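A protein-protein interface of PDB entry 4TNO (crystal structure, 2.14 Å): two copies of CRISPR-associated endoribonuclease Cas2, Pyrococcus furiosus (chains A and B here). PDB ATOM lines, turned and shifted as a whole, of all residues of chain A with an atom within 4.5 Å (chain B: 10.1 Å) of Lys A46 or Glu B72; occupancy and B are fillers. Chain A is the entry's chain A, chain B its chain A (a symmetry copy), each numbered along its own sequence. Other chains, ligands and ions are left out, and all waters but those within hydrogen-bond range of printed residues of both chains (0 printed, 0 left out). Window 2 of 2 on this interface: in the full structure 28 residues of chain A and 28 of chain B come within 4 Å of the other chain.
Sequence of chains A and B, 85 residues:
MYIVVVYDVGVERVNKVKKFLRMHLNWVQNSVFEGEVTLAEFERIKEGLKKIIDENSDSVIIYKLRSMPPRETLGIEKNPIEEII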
ATOM      1  N   PHE A  42      11.694  30.967  -9.466  1.00  0.00           N
ATOM      2  CA  PHE A  42      11.459  29.555  -9.165  1.00  0.00           C
ATOM      3  C   PHE A  42      12.259  28.641 -10.083  1.00  0.00           C
ATOM      4  O   PHE A  42      13.088  27.851  -9.613  1.00  0.00           O
ATOM      5  CB  PHE A  42       9.968  29.236  -9.275  1.00  0.00           C
ATOM      6  CG  PHE A  42       9.589  27.854  -8.806  1.00  0.00           C
ATOM      7  CD1 PHE A  42      10.488  27.050  -8.125  1.00  0.00           C
ATOM      8  CD2 PHE A  42       8.309  27.367  -9.038  1.00  0.00           C
ATOM      9  CE1 PHE A  42      10.125  25.781  -7.698  1.00  0.00           C
ATOM     10  CE2 PHE A  42       7.942  26.104  -8.613  1.00  0.00           C
ATOM     11  CZ  PHE A  42       8.856  25.311  -7.939  1.00  0.00           C
ATOM     12  N   GLU A  43      12.014  28.723 -11.389  1.00  0.00           N
ATOM     13  CA  GLU A  43      12.718  27.819 -12.291  1.00  0.00           C
ATOM     14  C   GLU A  43      14.153  28.291 -12.487  1.00  0.00           C
ATOM     15  O   GLU A  43      15.023  27.489 -12.865  1.00  0.00           O
ATOM     16  CB  GLU A  43      11.986  27.664 -13.625  1.00  0.00           C
ATOM     17  CG  GLU A  43      11.790  26.199 -13.997  1.00  0.00           C
ATOM     18  CD  GLU A  43      10.458  25.908 -14.673  1.00  0.00           C
ATOM     19  OE1 GLU A  43      10.410  25.959 -15.923  1.00  0.00           O
ATOM     20  OE2 GLU A  43       9.463  25.636 -13.951  1.00  0.00           O
ATOM     21  N   ARG A  44      14.417  29.560 -12.165  1.00  0.00           N
ATOM     22  CA  ARG A  44      15.798  30.021 -12.064  1.00  0.00           C
ATOM     23  C   ARG A  44      16.468  29.286 -10.896  1.00  0.00           C
ATOM     24  O   ARG A  44      17.538  28.684 -11.050  1.00  0.00           O
ATOM     25  CB  ARG A  44      15.885  31.544 -11.870  1.00  0.00           C
ATOM     26  CG  ARG A  44      15.394  32.444 -13.043  1.00  0.00           C
ATOM     27  CD  ARG A  44      15.421  31.755 -14.413  1.00  0.00           C
ATOM     28  NE  ARG A  44      14.784  32.559 -15.464  1.00  0.00           N
ATOM     29  CZ  ARG A  44      15.379  33.549 -16.135  1.00  0.00           C
ATOM     30  NH1 ARG A  44      16.639  33.877 -15.872  1.00  0.00           N
ATOM     31  NH2 ARG A  44      14.715  34.216 -17.076  1.00  0.00           N
ATOM     32  N   ILE A  45      15.836  29.340  -9.729  1.00  0.00           N
ATOM     33  CA  ILE A  45      16.318  28.627  -8.556  1.00  0.00           C
ATOM     34  C   ILE A  45      16.485  27.156  -8.876  1.00  0.00           C
ATOM     35  O   ILE A  45      17.536  26.558  -8.637  1.00  0.00           O
ATOM     36  CB  ILE A  45      15.344  28.788  -7.368  1.00  0.00           C
ATOM     37  CG1 ILE A  45      15.553  30.140  -6.689  1.00  0.00           C
ATOM     38  CG2 ILE A  45      15.550  27.698  -6.340  1.00  0.00           C
ATOM     39  CD1 ILE A  45      14.398  30.573  -5.843  1.00  0.00           C
ATOM     40  N   LYS A  46      15.435  26.590  -9.459  1.00  0.00           N
ATOM     41  CA  LYS A  46      15.325  25.148  -9.664  1.00  0.00           C
ATOM     42  C   LYS A  46      16.353  24.583 -10.640  1.00  0.00           C
ATOM     43  O   LYS A  46      17.054  23.627 -10.301  1.00  0.00           O
ATOM     44  CB  LYS A  46      13.919  24.796 -10.133  1.00  0.00           C
ATOM     45  CG  LYS A  46      13.827  23.486 -10.888  1.00  0.00           C
ATOM     46  CD  LYS A  46      12.462  23.321 -11.551  1.00  0.00           C
ATOM     47  CE  LYS A  46      12.130  21.853 -11.680  1.00  0.00           C
ATOM     48  NZ  LYS A  46      11.291  21.508 -12.863  1.00  0.00           N
ATOM     49  N   GLU A  47      16.457  25.152 -11.839  1.00  0.00           N
ATOM     50  CA  GLU A  47      17.495  24.674 -12.730  1.00  0.00           C
ATOM     51  C   GLU A  47      18.834  25.078 -12.169  1.00  0.00           C
ATOM     52  O   GLU A  47      19.737  24.249 -12.092  1.00  0.00           O
ATOM     53  CB  GLU A  47      17.327  25.191 -14.148  1.00  0.00           C
ATOM     54  CG  GLU A  47      18.472  24.719 -15.043  1.00  0.00           C
ATOM     55  CD  GLU A  47      18.036  23.725 -16.102  1.00  0.00           C
ATOM     56  OE1 GLU A  47      16.860  23.781 -16.533  1.00  0.00           O
ATOM     57  OE2 GLU A  47      18.866  22.866 -16.475  1.00  0.00           O
ATOM     58  N   GLY A  48      18.932  26.332 -11.734  1.00  0.00           N
ATOM     59  CA  GLY A  48      20.111  26.837 -11.053  1.00  0.00           C
ATOM     60  C   GLY A  48      20.655  25.831 -10.058  1.00  0.00           C
ATOM     61  O   GLY A  48      21.860  25.674  -9.924  1.00  0.00           O
ATOM     62  N   LEU A  49      19.758  25.113  -9.391  1.00  0.00           N
ATOM     63  CA  LEU A  49      20.161  24.081  -8.451  1.00  0.00           C
ATOM     64  C   LEU A  49      20.562  22.780  -9.137  1.00  0.00           C
ATOM     65  O   LEU A  49      21.439  22.070  -8.657  1.00  0.00           O
ATOM     66  CB  LEU A  49      19.030  23.812  -7.461  1.00  0.00           C
ATOM     67  CG  LEU A  49      18.931  24.711  -6.225  1.00  0.00           C
ATOM     68  CD1 LEU A  49      17.627  24.443  -5.482  1.00  0.00           C
ATOM     69  CD2 LEU A  49      20.099  24.463  -5.325  1.00  0.00           C
ATOM     70  N   LYS A  50      19.918  22.453 -10.256  1.00  0.00           N
ATOM     71  CA  LYS A  50      20.264  21.215 -10.978  1.00  0.00           C
ATOM     72  C   LYS A  50      21.678  21.273 -11.580  1.00  0.00           C
ATOM     73  O   LYS A  50      22.433  20.284 -11.503  1.00  0.00           O
ATOM     74  CB  LYS A  50      19.250  20.898 -12.079  1.00  0.00           C
ATOM     75  CG  LYS A  50      19.891  20.305 -13.337  1.00  0.00           C
ATOM     76  CD  LYS A  50      18.992  19.315 -14.057  1.00  0.00           C
ATOM     77  CE  LYS A  50      19.787  18.501 -15.102  1.00  0.00           C
ATOM     78  NZ  LYS A  50      20.760  19.323 -15.897  1.00  0.00           N
ATOM     79  N   VAL A  60      17.187  17.427  -3.337  1.00  0.00           N
ATOM     80  CA  VAL A  60      16.559  18.678  -2.952  1.00  0.00           C
ATOM     81  C   VAL A  60      15.064  18.456  -2.929  1.00  0.00           C
ATOM     82  O   VAL A  60      14.501  17.939  -3.898  1.00  0.00           O
ATOM     83  CB  VAL A  60      16.903  19.814  -3.930  1.00  0.00           C
ATOM     84  CG1 VAL A  60      16.212  21.104  -3.540  1.00  0.00           C
ATOM     85  CG2 VAL A  60      18.376  20.015  -3.963  1.00  0.00           C
ATOM     86  N   ILE A  61      14.426  18.778  -1.809  1.00  0.00           N
ATOM     87  CA  ILE A  61      12.985  18.881  -1.806  1.00  0.00           C
ATOM     88  C   ILE A  61      12.652  20.346  -1.730  1.00  0.00           C
ATOM     89  O   ILE A  61      13.126  21.073  -0.850  1.00  0.00           O
ATOM     90  CB  ILE A  61      12.321  18.154  -0.646  1.00  0.00           C
ATOM     91  CG1 ILE A  61      12.674  16.670  -0.685  1.00  0.00           C
ATOM     92  CG2 ILE A  61      10.809  18.339  -0.716  1.00  0.00           C
ATOM     93  CD1 ILE A  61      12.124  15.880   0.514  1.00  0.00           C
ATOM     94  N   ILE A  62      11.856  20.782  -2.687  1.00  0.00           N
ATOM     95  CA  ILE A  62      11.299  22.115  -2.642  1.00  0.00           C
ATOM     96  C   ILE A  62       9.830  22.007  -2.374  1.00  0.00           C
ATOM     97  O   ILE A  62       9.068  21.573  -3.230  1.00  0.00           O
ATOM     98  CB  ILE A  62      11.493  22.860  -3.930  1.00  0.00           C
ATOM     99  CG1 ILE A  62      12.948  22.766  -4.385  1.00  0.00           C
ATOM    100  CG2 ILE A  62      11.051  24.301  -3.749  1.00  0.00           C
ATOM    101  CD1 ILE A  62      13.196  23.543  -5.630  1.00  0.00           C
ATOM    102  N   LYS A  64       6.306  23.381  -2.303  1.00  0.00           N
ATOM    103  CA  LYS A  64       5.608  24.492  -2.977  1.00  0.00           C
ATOM    104  C   LYS A  64       4.341  24.911  -2.240  1.00  0.00           C
ATOM    105  O   LYS A  64       3.304  24.270  -2.345  1.00  0.00           O
ATOM    106  CB  LYS A  64       5.291  24.092  -4.408  1.00  0.00           C
ATOM    107  CG  LYS A  64       6.517  23.634  -5.134  1.00  0.00           C
ATOM    108  CD  LYS A  64       6.154  22.682  -6.253  1.00  0.00           C
ATOM    109  CE  LYS A  64       5.995  23.398  -7.591  1.00  0.00           C
ATOM    110  NZ  LYS A  64       7.025  22.958  -8.566  1.00  0.00           N
ATOM    111  N   VAL B  28      11.733  11.365   4.445  1.00  0.00           N
ATOM    112  CA  VAL B  28      11.796  11.636   3.002  1.00  0.00           C
ATOM    113  C   VAL B  28      13.144  12.129   2.482  1.00  0.00           C
ATOM    114  O   VAL B  28      13.397  12.102   1.280  1.00  0.00           O
ATOM    115  CB  VAL B  28      10.731  12.659   2.593  1.00  0.00           C
ATOM    116  CG1 VAL B  28       9.352  12.040   2.720  1.00  0.00           C
ATOM    117  CG2 VAL B  28      10.860  13.915   3.435  1.00  0.00           C
ATOM    118  N   GLN B  29      13.992  12.608   3.382  1.00  0.00           N
ATOM    119  CA  GLN B  29      15.340  13.033   3.033  1.00  0.00           C
ATOM    120  C   GLN B  29      16.101  12.995   4.324  1.00  0.00           C
ATOM    121  O   GLN B  29      15.488  12.957   5.395  1.00  0.00           O
ATOM    122  CB  GLN B  29      15.366  14.442   2.419  1.00  0.00           C
ATOM    123  CG  GLN B  29      16.726  14.901   1.871  1.00  0.00           C
ATOM    124  CD  GLN B  29      16.664  16.278   1.153  1.00  0.00           C
ATOM    125  OE1 GLN B  29      16.315  16.359  -0.027  1.00  0.00           O
ATOM    126  NE2 GLN B  29      17.010  17.348   1.870  1.00  0.00           N
ATOM    127  N   GLU B  34       7.966  14.080   7.408  1.00  0.00           N
ATOM    128  CA  GLU B  34       6.648  14.682   7.285  1.00  0.00           C
ATOM    129  C   GLU B  34       5.531  13.661   7.436  1.00  0.00           C
ATOM    130  O   GLU B  34       5.709  12.478   7.122  1.00  0.00           O
ATOM    131  CB  GLU B  34       6.505  15.394   5.939  1.00  0.00           C
ATOM    132  CG  GLU B  34       6.781  14.505   4.747  1.00  0.00           C
ATOM    133  CD  GLU B  34       6.490  15.217   3.408  1.00  0.00           C
ATOM    134  OE1 GLU B  34       7.420  15.400   2.589  1.00  0.00           O
ATOM    135  OE2 GLU B  34       5.322  15.599   3.176  1.00  0.00           O
ATOM    136  N   MET B  68      -1.035  17.930   3.537  1.00  0.00           N
ATOM    137  CA  MET B  68       0.177  17.556   2.832  1.00  0.00           C
ATOM    138  C   MET B  68       0.384  18.564   1.722  1.00  0.00           C
ATOM    139  O   MET B  68      -0.534  18.817   0.965  1.00  0.00           O
ATOM    140  CB  MET B  68       0.089  16.132   2.276  1.00  0.00           C
ATOM    141  CG  MET B  68       1.402  15.624   1.710  1.00  0.00           C
ATOM    142  SD  MET B  68       1.393  13.919   1.124  1.00  0.00           S
ATOM    143  CE  MET B  68       3.050  13.731   0.485  1.00  0.00           C
ATOM    144  N   PRO B  69       1.587  19.169   1.648  1.00  0.00           N
ATOM    145  CA  PRO B  69       1.902  20.138   0.586  1.00  0.00           C
ATOM    146  C   PRO B  69       2.412  19.511  -0.695  1.00  0.00           C
ATOM    147  O   PRO B  69       3.092  18.494  -0.653  1.00  0.00           O
ATOM    148  CB  PRO B  69       2.997  20.993   1.214  1.00  0.00           C
ATOM    149  CG  PRO B  69       3.657  20.080   2.165  1.00  0.00           C
ATOM    150  CD  PRO B  69       2.570  19.226   2.741  1.00  0.00           C
ATOM    151  N   PRO B  70       2.097  20.124  -1.841  1.00  0.00           N
ATOM    152  CA  PRO B  70       2.793  19.725  -3.060  1.00  0.00           C
ATOM    153  C   PRO B  70       4.273  20.058  -2.931  1.00  0.00           C
ATOM    154  O   PRO B  70       4.643  20.857  -2.075  1.00  0.00           O
ATOM    155  CB  PRO B  70       2.132  20.573  -4.135  1.00  0.00           C
ATOM    156  CG  PRO B  70       1.695  21.759  -3.418  1.00  0.00           C
ATOM    157  CD  PRO B  70       1.263  21.312  -2.057  1.00  0.00           C
ATOM    158  N   ARG B  71       5.095  19.479  -3.787  1.00  0.00           N
ATOM    159  CA  ARG B  71       6.534  19.549  -3.618  1.00  0.00           C
ATOM    160  C   ARG B  71       7.141  19.374  -4.987  1.00  0.00           C
ATOM    161  O   ARG B  71       6.459  18.982  -5.922  1.00  0.00           O
ATOM    162  CB  ARG B  71       7.007  18.421  -2.714  1.00  0.00           C
ATOM    163  CG  ARG B  71       6.516  17.129  -3.336  1.00  0.00           C
ATOM    164  CD  ARG B  71       6.331  16.066  -2.339  1.00  0.00           C
ATOM    165  NE  ARG B  71       5.469  16.521  -1.256  1.00  0.00           N
ATOM    166  CZ  ARG B  71       5.766  16.295   0.016  1.00  0.00           C
ATOM    167  NH1 ARG B  71       6.898  15.655   0.292  1.00  0.00           N
ATOM    168  NH2 ARG B  71       4.986  16.742   1.008  1.00  0.00           N
ATOM    169  N   GLU B  72       8.432  19.612  -5.115  1.00  0.00           N
ATOM    170  CA  GLU B  72       9.134  19.075  -6.265  1.00  0.00           C
ATOM    171  C   GLU B  72      10.504  18.599  -5.796  1.00  0.00           C
ATOM    172  O   GLU B  72      11.027  19.092  -4.800  1.00  0.00           O
ATOM    173  CB  GLU B  72       9.236  20.102  -7.391  1.00  0.00           C
ATOM    174  CG  GLU B  72       9.499  19.469  -8.761  1.00  0.00           C
ATOM    175  CD  GLU B  72       9.288  20.432  -9.923  1.00  0.00           C
ATOM    176  OE1 GLU B  72       8.634  21.487  -9.742  1.00  0.00           O
ATOM    177  OE2 GLU B  72       9.786  20.126 -11.024  1.00  0.00           O
ATOM    178  N   THR B  73      11.062  17.615  -6.487  1.00  0.00           N
ATOM    179  CA  THR B  73      12.234  16.916  -5.984  1.00  0.00           C
ATOM    180  C   THR B  73      13.308  16.778  -7.050  1.00  0.00           C
ATOM    181  O   THR B  73      13.058  16.266  -8.145  1.00  0.00           O
ATOM    182  CB  THR B  73      11.873  15.508  -5.468  1.00  0.00           C
ATOM    183  OG1 THR B  73      11.234  14.766  -6.515  1.00  0.00           O
ATOM    184  CG2 THR B  73      10.935  15.595  -4.297  1.00  0.00           C
ATOM    185  N   LEU B  74      14.508  17.244  -6.718  1.00  0.00           N
ATOM    186  CA  LEU B  74      15.659  17.089  -7.592  1.00  0.00           C
ATOM    187  C   LEU B  74      16.533  15.971  -7.073  1.00  0.00           C
ATOM    188  O   LEU B  74      16.692  15.816  -5.855  1.00  0.00           O
ATOM    189  CB  LEU B  74      16.473  18.378  -7.675  1.00  0.00           C
ATOM    190  CG  LEU B  74      15.710  19.633  -8.084  1.00  0.00           C
ATOM    191  CD1 LEU B  74      16.658  20.819  -8.130  1.00  0.00           C
ATOM    192  CD2 LEU B  74      15.031  19.423  -9.429  1.00  0.00           C
ATOM    193  N   GLY B  75      17.086  15.194  -8.000  1.00  0.00           N
ATOM    194  CA  GLY B  75      18.080  14.194  -7.672  1.00  0.00           C
ATOM    195  C   GLY B  75      17.525  12.925  -7.065  1.00  0.00           C
ATOM    196  O   GLY B  75      16.332  12.612  -7.200  1.00  0.00           O
ATOM    197  N   ILE B  76      18.411  12.197  -6.390  1.00  0.00           N
ATOM    198  CA  ILE B  76      18.084  10.910  -5.791  1.00  0.00           C
ATOM    199  C   ILE B  76      16.921  11.042  -4.807  1.00  0.00           C
ATOM    200  O   ILE B  76      17.101  11.506  -3.672  1.00  0.00           O
ATOM    201  CB  ILE B  76      19.335  10.286  -5.083  1.00  0.00           C
ATOM    202  CG1 ILE B  76      18.942   9.194  -4.086  1.00  0.00           C
ATOM    203  CG2 ILE B  76      20.161  11.337  -4.365  1.00  0.00           C
ATOM    204  CD1 ILE B  76      20.134   8.522  -3.442  1.00  0.00           C
ATOM    205  N   GLU B  77      15.722  10.677  -5.265  1.00  0.00           N
ATOM    206  CA  GLU B  77      14.567  10.581  -4.376  1.00  0.00           C
ATOM    207  C   GLU B  77      14.742   9.359  -3.502  1.00  0.00           C
ATOM    208  O   GLU B  77      15.226   8.328  -3.956  1.00  0.00           O
ATOM    209  CB  GLU B  77      13.251  10.493  -5.148  1.00  0.00           C
ATOM    210  CG  GLU B  77      12.785  11.791  -5.770  1.00  0.00           C
ATOM    211  CD  GLU B  77      11.320  11.741  -6.109  1.00  0.00           C
ATOM    212  OE1 GLU B  77      10.550  11.191  -5.292  1.00  0.00           O
ATOM    213  OE2 GLU B  77      10.935  12.220  -7.200  1.00  0.00           O
ATOM    214  N   ILE B  81       6.715   9.457  -3.693  1.00  0.00           N
ATOM    215  CA  ILE B  81       5.555  10.123  -3.117  1.00  0.00           C
ATOM    216  C   ILE B  81       4.461   9.153  -2.697  1.00  0.00           C
ATOM    217  O   ILE B  81       3.728   9.389  -1.721  1.00  0.00           O
ATOM    218  CB  ILE B  81       4.946  11.117  -4.111  1.00  0.00           C
ATOM    219  CG1 ILE B  81       6.039  11.754  -4.992  1.00  0.00           C
ATOM    220  CG2 ILE B  81       4.089  12.137  -3.373  1.00  0.00           C
ATOM    221  CD1 ILE B  81       7.082  12.582  -4.251  1.00  0.00           C
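Hydrophobic or aromatic side chains of chain A within 4 Å of the printed part of chain B: Leu A49, Ile A61 and Ile A62.
Among the printed residues, Asp or Glu carboxylates within 4 Å of a Lys or Arg side-chain nitrogen of the other chain: Lys A46 with Glu B72 and Lys A64 with Glu B72.
N of Leu B74 lies within hydrogen-bond range of O of Val A60, at 2.9 Å.
The backbone carbonyl oxygen (O) of Ile A62 sits at hydrogen-bond distance from the backbone NH (N) of Glu B72 (2.8 Å).
O of Pro B70 sits at hydrogen-bond distance from N of Lys A64 (3.0 Å).
The side-chain carboxylate (OE2) of Glu B72 is in salt-bridge range of the side-chain amino group (NZ) of Lys A46 (2.7 Å).
The side-chain amino group (NZ) of Lys A64 is in salt-bridge range of the side-chain carboxylate (OE1) of Glu B72 (2.5 Å).
No residue of chain B comes within 4 Å of Glu A43.
Of chain B, only Leu B74 (3.9 Å) comes within 4 Å of Leu A49.
Printed residues of chain A within 4 Å of Pro B70: Lys A64.
Of the printed residues of chain A, Leu B74 touches Lys A46 (3.6 Å), Leu A49 (3.9 Å) and Val A60 (2.9 Å).
No position is printed for both chains.
Of the 15 pairs that touch across the chains among the printed residues, none has its exchanged pair printed and touching as well.
Lys A46 touches Leu B74 (O to CD1, 3.6 Å).
Leu A49 touches Leu B74 (CB to CD1, 3.9 Å).
Gln B29 touches Val A60.
Val A60 touches Glu B72 (O to O, 3.8 Å).
Thr B73 touches Val A60 (CA to O, 3.2 Å).
CG2 of Val B28 touches CD1 of Ile A61, at 3.7 Å.
Ile A61 touches Gln B29.
CA of Ile A61 touches O of Glu B72 (3.6 Å).
Arg B71 touches Ile A62.
CD of Lys A64 touches C of Arg B71, 3.7 Å away.
O of Pro B69 sits at hydrogen-bond distance from NH2 of Arg B71 (3.1 Å).
NH2 of Arg B71 lies within salt-bridge range of OE2 of Glu B34 (2.5 Å).
The side-chain hydroxyl (OG1) of Thr B73 sits at hydrogen-bond distance from the side-chain carboxylate (OE2) of Glu B77 (2.7 Å).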
